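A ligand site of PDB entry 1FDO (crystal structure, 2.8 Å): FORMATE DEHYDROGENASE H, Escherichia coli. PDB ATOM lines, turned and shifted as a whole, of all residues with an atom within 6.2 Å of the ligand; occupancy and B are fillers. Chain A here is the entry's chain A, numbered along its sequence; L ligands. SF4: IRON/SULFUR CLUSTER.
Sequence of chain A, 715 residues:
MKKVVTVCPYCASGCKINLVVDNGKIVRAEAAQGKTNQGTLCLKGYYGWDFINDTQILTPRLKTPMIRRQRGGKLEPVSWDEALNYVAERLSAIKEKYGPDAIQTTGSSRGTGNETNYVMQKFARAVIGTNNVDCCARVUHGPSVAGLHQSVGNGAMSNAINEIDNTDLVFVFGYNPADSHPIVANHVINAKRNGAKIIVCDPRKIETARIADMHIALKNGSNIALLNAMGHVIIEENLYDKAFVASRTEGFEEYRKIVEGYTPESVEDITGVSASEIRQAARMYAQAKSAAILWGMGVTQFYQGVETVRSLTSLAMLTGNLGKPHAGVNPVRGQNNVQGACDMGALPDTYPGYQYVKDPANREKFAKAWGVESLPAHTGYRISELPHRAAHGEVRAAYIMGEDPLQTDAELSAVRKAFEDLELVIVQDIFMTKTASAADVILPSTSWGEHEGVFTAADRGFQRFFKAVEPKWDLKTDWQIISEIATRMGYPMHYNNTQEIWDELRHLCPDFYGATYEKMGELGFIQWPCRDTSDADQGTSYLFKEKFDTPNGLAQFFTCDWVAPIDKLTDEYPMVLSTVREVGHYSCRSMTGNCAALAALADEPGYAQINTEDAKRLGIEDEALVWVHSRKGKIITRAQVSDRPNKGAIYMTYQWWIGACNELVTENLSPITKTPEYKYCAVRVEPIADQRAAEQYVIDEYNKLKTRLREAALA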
ATOM      1  N   CYS A   8     -19.182 -30.159 -29.135  1.00  0.00           N
ATOM      2  CA  CYS A   8     -19.437 -30.287 -27.707  1.00  0.00           C
ATOM      3  C   CYS A   8     -20.931 -30.432 -27.373  1.00  0.00           C
ATOM      4  O   CYS A   8     -21.763 -29.666 -27.870  1.00  0.00           O
ATOM      5  CB  CYS A   8     -18.814 -29.120 -26.944  1.00  0.00           C
ATOM      6  SG  CYS A   8     -19.142 -29.147 -25.148  1.00  0.00           S
ATOM      7  N   PRO A   9     -21.280 -31.432 -26.542  1.00  0.00           N
ATOM      8  CA  PRO A   9     -22.631 -31.791 -26.061  1.00  0.00           C
ATOM      9  C   PRO A   9     -23.180 -30.923 -24.914  1.00  0.00           C
ATOM     10  O   PRO A   9     -24.246 -31.206 -24.382  1.00  0.00           O
ATOM     11  CB  PRO A   9     -22.441 -33.228 -25.573  1.00  0.00           C
ATOM     12  CG  PRO A   9     -21.078 -33.170 -24.989  1.00  0.00           C
ATOM     13  CD  PRO A   9     -20.305 -32.427 -26.068  1.00  0.00           C
ATOM     14  N   TYR A  10     -22.468 -29.869 -24.564  1.00  0.00           N
ATOM     15  CA  TYR A  10     -22.895 -29.040 -23.468  1.00  0.00           C
ATOM     16  C   TYR A  10     -23.669 -27.878 -23.995  1.00  0.00           C
ATOM     17  O   TYR A  10     -24.820 -28.077 -24.375  1.00  0.00           O
ATOM     18  CB  TYR A  10     -21.713 -28.680 -22.571  1.00  0.00           C
ATOM     19  CG  TYR A  10     -21.251 -29.894 -21.811  1.00  0.00           C
ATOM     20  CD1 TYR A  10     -22.086 -30.480 -20.876  1.00  0.00           C
ATOM     21  CD2 TYR A  10     -20.043 -30.519 -22.083  1.00  0.00           C
ATOM     22  CE1 TYR A  10     -21.745 -31.670 -20.251  1.00  0.00           C
ATOM     23  CE2 TYR A  10     -19.676 -31.735 -21.456  1.00  0.00           C
ATOM     24  CZ  TYR A  10     -20.547 -32.287 -20.542  1.00  0.00           C
ATOM     25  OH  TYR A  10     -20.271 -33.455 -19.880  1.00  0.00           O
ATOM     26  N   CYS A  11     -23.070 -26.695 -24.091  1.00  0.00           N
ATOM     27  CA  CYS A  11     -23.850 -25.571 -24.597  1.00  0.00           C
ATOM     28  C   CYS A  11     -24.005 -25.448 -26.122  1.00  0.00           C
ATOM     29  O   CYS A  11     -23.496 -26.269 -26.875  1.00  0.00           O
ATOM     30  CB  CYS A  11     -23.422 -24.273 -23.913  1.00  0.00           C
ATOM     31  SG  CYS A  11     -22.016 -23.363 -24.598  1.00  0.00           S
ATOM     32  N   ALA A  12     -24.821 -24.512 -26.585  1.00  0.00           N
ATOM     33  CA  ALA A  12     -25.048 -24.334 -28.025  1.00  0.00           C
ATOM     34  C   ALA A  12     -23.996 -23.506 -28.749  1.00  0.00           C
ATOM     35  O   ALA A  12     -24.234 -23.029 -29.848  1.00  0.00           O
ATOM     36  CB  ALA A  12     -26.410 -23.731 -28.266  1.00  0.00           C
ATOM     37  N   SER A  13     -22.810 -23.354 -28.160  1.00  0.00           N
ATOM     38  CA  SER A  13     -21.770 -22.593 -28.813  1.00  0.00           C
ATOM     39  C   SER A  13     -21.331 -23.374 -30.051  1.00  0.00           C
ATOM     40  O   SER A  13     -20.853 -22.792 -31.010  1.00  0.00           O
ATOM     41  CB  SER A  13     -20.594 -22.363 -27.877  1.00  0.00           C
ATOM     42  OG  SER A  13     -21.021 -21.687 -26.690  1.00  0.00           O
ATOM     43  N   GLY A  14     -21.491 -24.693 -29.995  1.00  0.00           N
ATOM     44  CA  GLY A  14     -21.151 -25.542 -31.117  1.00  0.00           C
ATOM     45  C   GLY A  14     -19.670 -25.715 -31.340  1.00  0.00           C
ATOM     46  O   GLY A  14     -19.200 -25.829 -32.492  1.00  0.00           O
ATOM     47  N   CYS A  15     -18.933 -25.729 -30.235  1.00  0.00           N
ATOM     48  CA  CYS A  15     -17.477 -25.903 -30.292  1.00  0.00           C
ATOM     49  C   CYS A  15     -17.104 -27.282 -30.843  1.00  0.00           C
ATOM     50  O   CYS A  15     -17.690 -28.290 -30.456  1.00  0.00           O
ATOM     51  CB  CYS A  15     -16.855 -25.702 -28.909  1.00  0.00           C
ATOM     52  SG  CYS A  15     -17.001 -24.007 -28.229  1.00  0.00           S
ATOM     53  N   ILE A  17     -14.556 -30.348 -31.267  1.00  0.00           N
ATOM     54  CA  ILE A  17     -13.561 -31.029 -30.440  1.00  0.00           C
ATOM     55  C   ILE A  17     -12.905 -32.194 -31.186  1.00  0.00           C
ATOM     56  O   ILE A  17     -13.528 -32.818 -32.068  1.00  0.00           O
ATOM     57  CB  ILE A  17     -14.261 -31.658 -29.197  1.00  0.00           C
ATOM     58  CG1 ILE A  17     -14.635 -30.588 -28.193  1.00  0.00           C
ATOM     59  CG2 ILE A  17     -13.391 -32.747 -28.528  1.00  0.00           C
ATOM     60  CD1 ILE A  17     -15.235 -31.204 -26.939  1.00  0.00           C
ATOM     61  N   ASN A  37     -15.648 -21.726 -32.154  1.00  0.00           N
ATOM     62  CA  ASN A  37     -14.581 -21.783 -31.167  1.00  0.00           C
ATOM     63  C   ASN A  37     -13.157 -21.631 -31.658  1.00  0.00           C
ATOM     64  O   ASN A  37     -12.291 -21.298 -30.867  1.00  0.00           O
ATOM     65  CB  ASN A  37     -14.646 -23.093 -30.399  1.00  0.00           C
ATOM     66  CG  ASN A  37     -14.264 -24.261 -31.237  1.00  0.00           C
ATOM     67  OD1 ASN A  37     -14.617 -24.294 -32.415  1.00  0.00           O
ATOM     68  ND2 ASN A  37     -13.526 -25.199 -30.681  1.00  0.00           N
ATOM     69  N   THR A  40     -10.487 -23.115 -29.336  1.00  0.00           N
ATOM     70  CA  THR A  40     -10.669 -22.939 -27.923  1.00  0.00           C
ATOM     71  C   THR A  40     -11.838 -23.761 -27.423  1.00  0.00           C
ATOM     72  O   THR A  40     -12.687 -24.186 -28.198  1.00  0.00           O
ATOM     73  CB  THR A  40     -10.929 -21.503 -27.573  1.00  0.00           C
ATOM     74  OG1 THR A  40     -12.261 -21.146 -27.990  1.00  0.00           O
ATOM     75  CG2 THR A  40      -9.928 -20.631 -28.233  1.00  0.00           C
ATOM     76  N   LEU A  41     -11.868 -23.967 -26.120  1.00  0.00           N
ATOM     77  CA  LEU A  41     -12.922 -24.695 -25.426  1.00  0.00           C
ATOM     78  C   LEU A  41     -12.881 -24.149 -24.010  1.00  0.00           C
ATOM     79  O   LEU A  41     -11.923 -23.482 -23.609  1.00  0.00           O
ATOM     80  CB  LEU A  41     -12.614 -26.193 -25.367  1.00  0.00           C
ATOM     81  CG  LEU A  41     -12.641 -27.064 -26.615  1.00  0.00           C
ATOM     82  CD1 LEU A  41     -12.086 -28.427 -26.257  1.00  0.00           C
ATOM     83  CD2 LEU A  41     -14.073 -27.186 -27.155  1.00  0.00           C
ATOM     84  N   CYS A  42     -13.916 -24.452 -23.252  1.00  0.00           N
ATOM     85  CA  CYS A  42     -13.966 -24.017 -21.868  1.00  0.00           C
ATOM     86  C   CYS A  42     -13.794 -25.284 -21.041  1.00  0.00           C
ATOM     87  O   CYS A  42     -13.803 -26.371 -21.588  1.00  0.00           O
ATOM     88  CB  CYS A  42     -15.303 -23.340 -21.568  1.00  0.00           C
ATOM     89  SG  CYS A  42     -16.684 -24.497 -21.424  1.00  0.00           S
ATOM     90  N   LEU A  43     -13.630 -25.128 -19.735  1.00  0.00           N
ATOM     91  CA  LEU A  43     -13.451 -26.235 -18.794  1.00  0.00           C
ATOM     92  C   LEU A  43     -14.317 -27.459 -19.095  1.00  0.00           C
ATOM     93  O   LEU A  43     -13.821 -28.570 -19.127  1.00  0.00           O
ATOM     94  CB  LEU A  43     -13.751 -25.749 -17.372  1.00  0.00           C
ATOM     95  CG  LEU A  43     -13.046 -26.359 -16.156  1.00  0.00           C
ATOM     96  CD1 LEU A  43     -11.719 -25.679 -15.958  1.00  0.00           C
ATOM     97  CD2 LEU A  43     -13.923 -26.172 -14.908  1.00  0.00           C
ATOM     98  N   LYS A  44     -15.610 -27.270 -19.304  1.00  0.00           N
ATOM     99  CA  LYS A  44     -16.508 -28.405 -19.577  1.00  0.00           C
ATOM    100  C   LYS A  44     -16.190 -29.142 -20.879  1.00  0.00           C
ATOM    101  O   LYS A  44     -16.143 -30.372 -20.909  1.00  0.00           O
ATOM    102  CB  LYS A  44     -17.968 -27.944 -19.613  1.00  0.00           C
ATOM    103  CG  LYS A  44     -18.550 -27.548 -18.260  1.00  0.00           C
ATOM    104  CD  LYS A  44     -19.899 -26.889 -18.443  1.00  0.00           C
ATOM    105  CE  LYS A  44     -19.735 -25.741 -19.420  1.00  0.00           C
ATOM    106  NZ  LYS A  44     -20.983 -24.983 -19.582  1.00  0.00           N
ATOM    107  N   GLY A  45     -15.987 -28.413 -21.964  1.00  0.00           N
ATOM    108  CA  GLY A  45     -15.684 -29.068 -23.212  1.00  0.00           C
ATOM    109  C   GLY A  45     -14.417 -29.882 -23.038  1.00  0.00           C
ATOM    110  O   GLY A  45     -14.374 -31.034 -23.451  1.00  0.00           O
ATOM    111  N   TYR A  46     -13.447 -29.297 -22.335  1.00  0.00           N
ATOM    112  CA  TYR A  46     -12.123 -29.890 -22.070  1.00  0.00           C
ATOM    113  C   TYR A  46     -12.123 -31.061 -21.103  1.00  0.00           C
ATOM    114  O   TYR A  46     -11.481 -32.068 -21.357  1.00  0.00           O
ATOM    115  CB  TYR A  46     -11.186 -28.820 -21.507  1.00  0.00           C
ATOM    116  CG  TYR A  46      -9.712 -28.983 -21.824  1.00  0.00           C
ATOM    117  CD1 TYR A  46      -8.863 -29.766 -21.002  1.00  0.00           C
ATOM    118  CD2 TYR A  46      -9.141 -28.297 -22.909  1.00  0.00           C
ATOM    119  CE1 TYR A  46      -7.473 -29.859 -21.265  1.00  0.00           C
ATOM    120  CE2 TYR A  46      -7.776 -28.378 -23.175  1.00  0.00           C
ATOM    121  CZ  TYR A  46      -6.939 -29.155 -22.355  1.00  0.00           C
ATOM    122  OH  TYR A  46      -5.574 -29.172 -22.624  1.00  0.00           O
ATOM    123  N   SER A 180     -22.750 -19.103 -19.613  1.00  0.00           N
ATOM    124  CA  SER A 180     -23.669 -19.909 -20.389  1.00  0.00           C
ATOM    125  C   SER A 180     -23.109 -20.357 -21.719  1.00  0.00           C
ATOM    126  O   SER A 180     -23.432 -21.443 -22.176  1.00  0.00           O
ATOM    127  CB  SER A 180     -24.906 -19.083 -20.621  1.00  0.00           C
ATOM    128  OG  SER A 180     -25.162 -18.300 -19.483  1.00  0.00           O
ATOM    129  N   HIS A 181     -22.427 -19.465 -22.412  1.00  0.00           N
ATOM    130  CA  HIS A 181     -21.845 -19.793 -23.698  1.00  0.00           C
ATOM    131  C   HIS A 181     -20.513 -19.041 -23.735  1.00  0.00           C
ATOM    132  O   HIS A 181     -20.443 -17.923 -24.260  1.00  0.00           O
ATOM    133  CB  HIS A 181     -22.739 -19.341 -24.859  1.00  0.00           C
ATOM    134  CG  HIS A 181     -24.164 -19.819 -24.782  1.00  0.00           C
ATOM    135  ND1 HIS A 181     -25.182 -19.056 -24.238  1.00  0.00           N
ATOM    136  CD2 HIS A 181     -24.743 -20.952 -25.220  1.00  0.00           C
ATOM    137  CE1 HIS A 181     -26.324 -19.704 -24.340  1.00  0.00           C
ATOM    138  NE2 HIS A 181     -26.095 -20.857 -24.939  1.00  0.00           N
ATOM    139  N   PRO A 182     -19.460 -19.602 -23.127  1.00  0.00           N
ATOM    140  CA  PRO A 182     -18.128 -19.016 -23.073  1.00  0.00           C
ATOM    141  C   PRO A 182     -17.517 -18.624 -24.401  1.00  0.00           C
ATOM    142  O   PRO A 182     -16.773 -17.637 -24.464  1.00  0.00           O
ATOM    143  CB  PRO A 182     -17.335 -20.090 -22.369  1.00  0.00           C
ATOM    144  CG  PRO A 182     -18.297 -20.525 -21.353  1.00  0.00           C
ATOM    145  CD  PRO A 182     -19.545 -20.729 -22.189  1.00  0.00           C
ATOM    146  N   ILE A 183     -17.794 -19.400 -25.456  1.00  0.00           N
ATOM    147  CA  ILE A 183     -17.302 -19.108 -26.802  1.00  0.00           C
ATOM    148  C   ILE A 183     -18.123 -17.983 -27.409  1.00  0.00           C
ATOM    149  O   ILE A 183     -17.638 -17.221 -28.241  1.00  0.00           O
ATOM    150  CB  ILE A 183     -17.258 -20.399 -27.708  1.00  0.00           C
ATOM    151  CG1 ILE A 183     -15.851 -21.019 -27.683  1.00  0.00           C
ATOM    152  CG2 ILE A 183     -17.682 -20.100 -29.139  1.00  0.00           C
ATOM    153  CD1 ILE A 183     -15.314 -21.400 -26.278  1.00  0.00           C
ATOM    154  N   VAL A 184     -19.365 -17.837 -26.944  1.00  0.00           N
ATOM    155  CA  VAL A 184     -20.219 -16.740 -27.417  1.00  0.00           C
ATOM    156  C   VAL A 184     -19.735 -15.507 -26.615  1.00  0.00           C
ATOM    157  O   VAL A 184     -19.707 -14.378 -27.141  1.00  0.00           O
ATOM    158  CB  VAL A 184     -21.757 -17.025 -27.203  1.00  0.00           C
ATOM    159  CG1 VAL A 184     -22.583 -15.741 -27.328  1.00  0.00           C
ATOM    160  CG2 VAL A 184     -22.252 -18.016 -28.258  1.00  0.00           C
ATOM    161  N   TYR A 586     -23.395 -28.560 -15.918  1.00  0.00           N
ATOM    162  CA  TYR A 586     -24.418 -28.315 -16.941  1.00  0.00           C
ATOM    163  C   TYR A 586     -25.779 -29.004 -16.764  1.00  0.00           C
ATOM    164  O   TYR A 586     -25.876 -30.227 -16.875  1.00  0.00           O
ATOM    165  CB  TYR A 586     -23.833 -28.661 -18.314  1.00  0.00           C
ATOM    166  CG  TYR A 586     -24.688 -28.221 -19.458  1.00  0.00           C
ATOM    167  CD1 TYR A 586     -25.764 -29.001 -19.878  1.00  0.00           C
ATOM    168  CD2 TYR A 586     -24.485 -26.991 -20.079  1.00  0.00           C
ATOM    169  CE1 TYR A 586     -26.618 -28.573 -20.893  1.00  0.00           C
ATOM    170  CE2 TYR A 586     -25.341 -26.548 -21.094  1.00  0.00           C
ATOM    171  CZ  TYR A 586     -26.403 -27.358 -21.484  1.00  0.00           C
ATOM    172  OH  TYR A 586     -27.284 -26.919 -22.444  1.00  0.00           O
HETATM  173 FE1  SF4 L   1     -17.830 -24.776 -23.482  1.00  0.00          FE
HETATM  174 FE2  SF4 L   1     -18.844 -26.856 -24.911  1.00  0.00          FE
HETATM  175 FE3  SF4 L   1     -17.884 -24.768 -26.314  1.00  0.00          FE
HETATM  176 FE4  SF4 L   1     -19.998 -24.559 -24.671  1.00  0.00          FE
HETATM  177  S1  SF4 L   1     -19.855 -25.774 -26.646  1.00  0.00           S
HETATM  178  S2  SF4 L   1     -18.396 -23.002 -24.812  1.00  0.00           S
HETATM  179  S3  SF4 L   1     -19.667 -26.088 -22.958  1.00  0.00           S
HETATM  180  S4  SF4 L   1     -16.669 -26.148 -24.929  1.00  0.00           S
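A sulfur (S1) of the ligand sits close to the backbone NH of Cys 15. SG of Cys 15 binds FE3 of the ligand (2.2 Å). SG of Cys 8 is bound to FE2 of the ligand, 2.3 Å away. N of Cys 11 lies close to S3 of the ligand (3.6 Å). The side-chain sulfur (SG) of Cys 11 is bound to an iron atom (FE4) of the ligand (2.3 Å). The backbone NH of Cys 42 lies close to a sulfur (S4) of the ligand (3.6 Å). An iron atom (FE1) of the ligand is bound by the side-chain sulfur (SG) of Cys 42 (2.4 Å). A sulfur (S2) of the ligand sits close to the side-chain hydroxyl (OG) of Ser 13 (3.5 Å). N of Gly 45 lies close to S4 of the ligand, at 3.8 Å. The side-chain amino group (NZ) of Lys 44 sits close to a sulfur (S3) of the ligand, 3.8 Å away. N of Ile 183 sits close to S2 of the ligand (3.7 Å).
The backbone carbonyl oxygen (O) of Cys 15 lies within hydrogen-bond range of the backbone NH (N) of Cys 8 (2.7 Å). The backbone NH (N) of Tyr 10 sits close to the side-chain sulfur (SG) of Cys 8 (3.5 Å). OG of Ser 13 sits close to SG of Cys 11. The backbone carbonyl oxygen of Ser 180 sits close to the side-chain sulfur of Cys 11. The backbone NH of Lys 44 sits close to the side-chain sulfur of Cys 42 (3.7 Å). The backbone carbonyl oxygen (O) of Tyr 10 sits at hydrogen-bond distance from the side-chain hydroxyl (OH) of Tyr 586, 3.3 Å away.
Tyr 10 touches the ligand (CB to S3, 3.3 Å). Gly 14 touches the ligand. Leu 41 touches the ligand. Pro 182 touches the ligand (CD to S2, 3.7 Å). Hydrophobic or aromatic side chains within 4 Å of the ligand: Tyr 10, Leu 41, Pro 182 and Ile 183. Within 4 Å of the ligand: Cys 8, Tyr 10, Cys 11, Ser 13, Gly 14, Cys 15, Leu 41, Cys 42, Lys 44, Gly 45, Pro 182 and Ile 183. Along chain A the residues within 4 Å of the ligand span positions 8 to 183.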
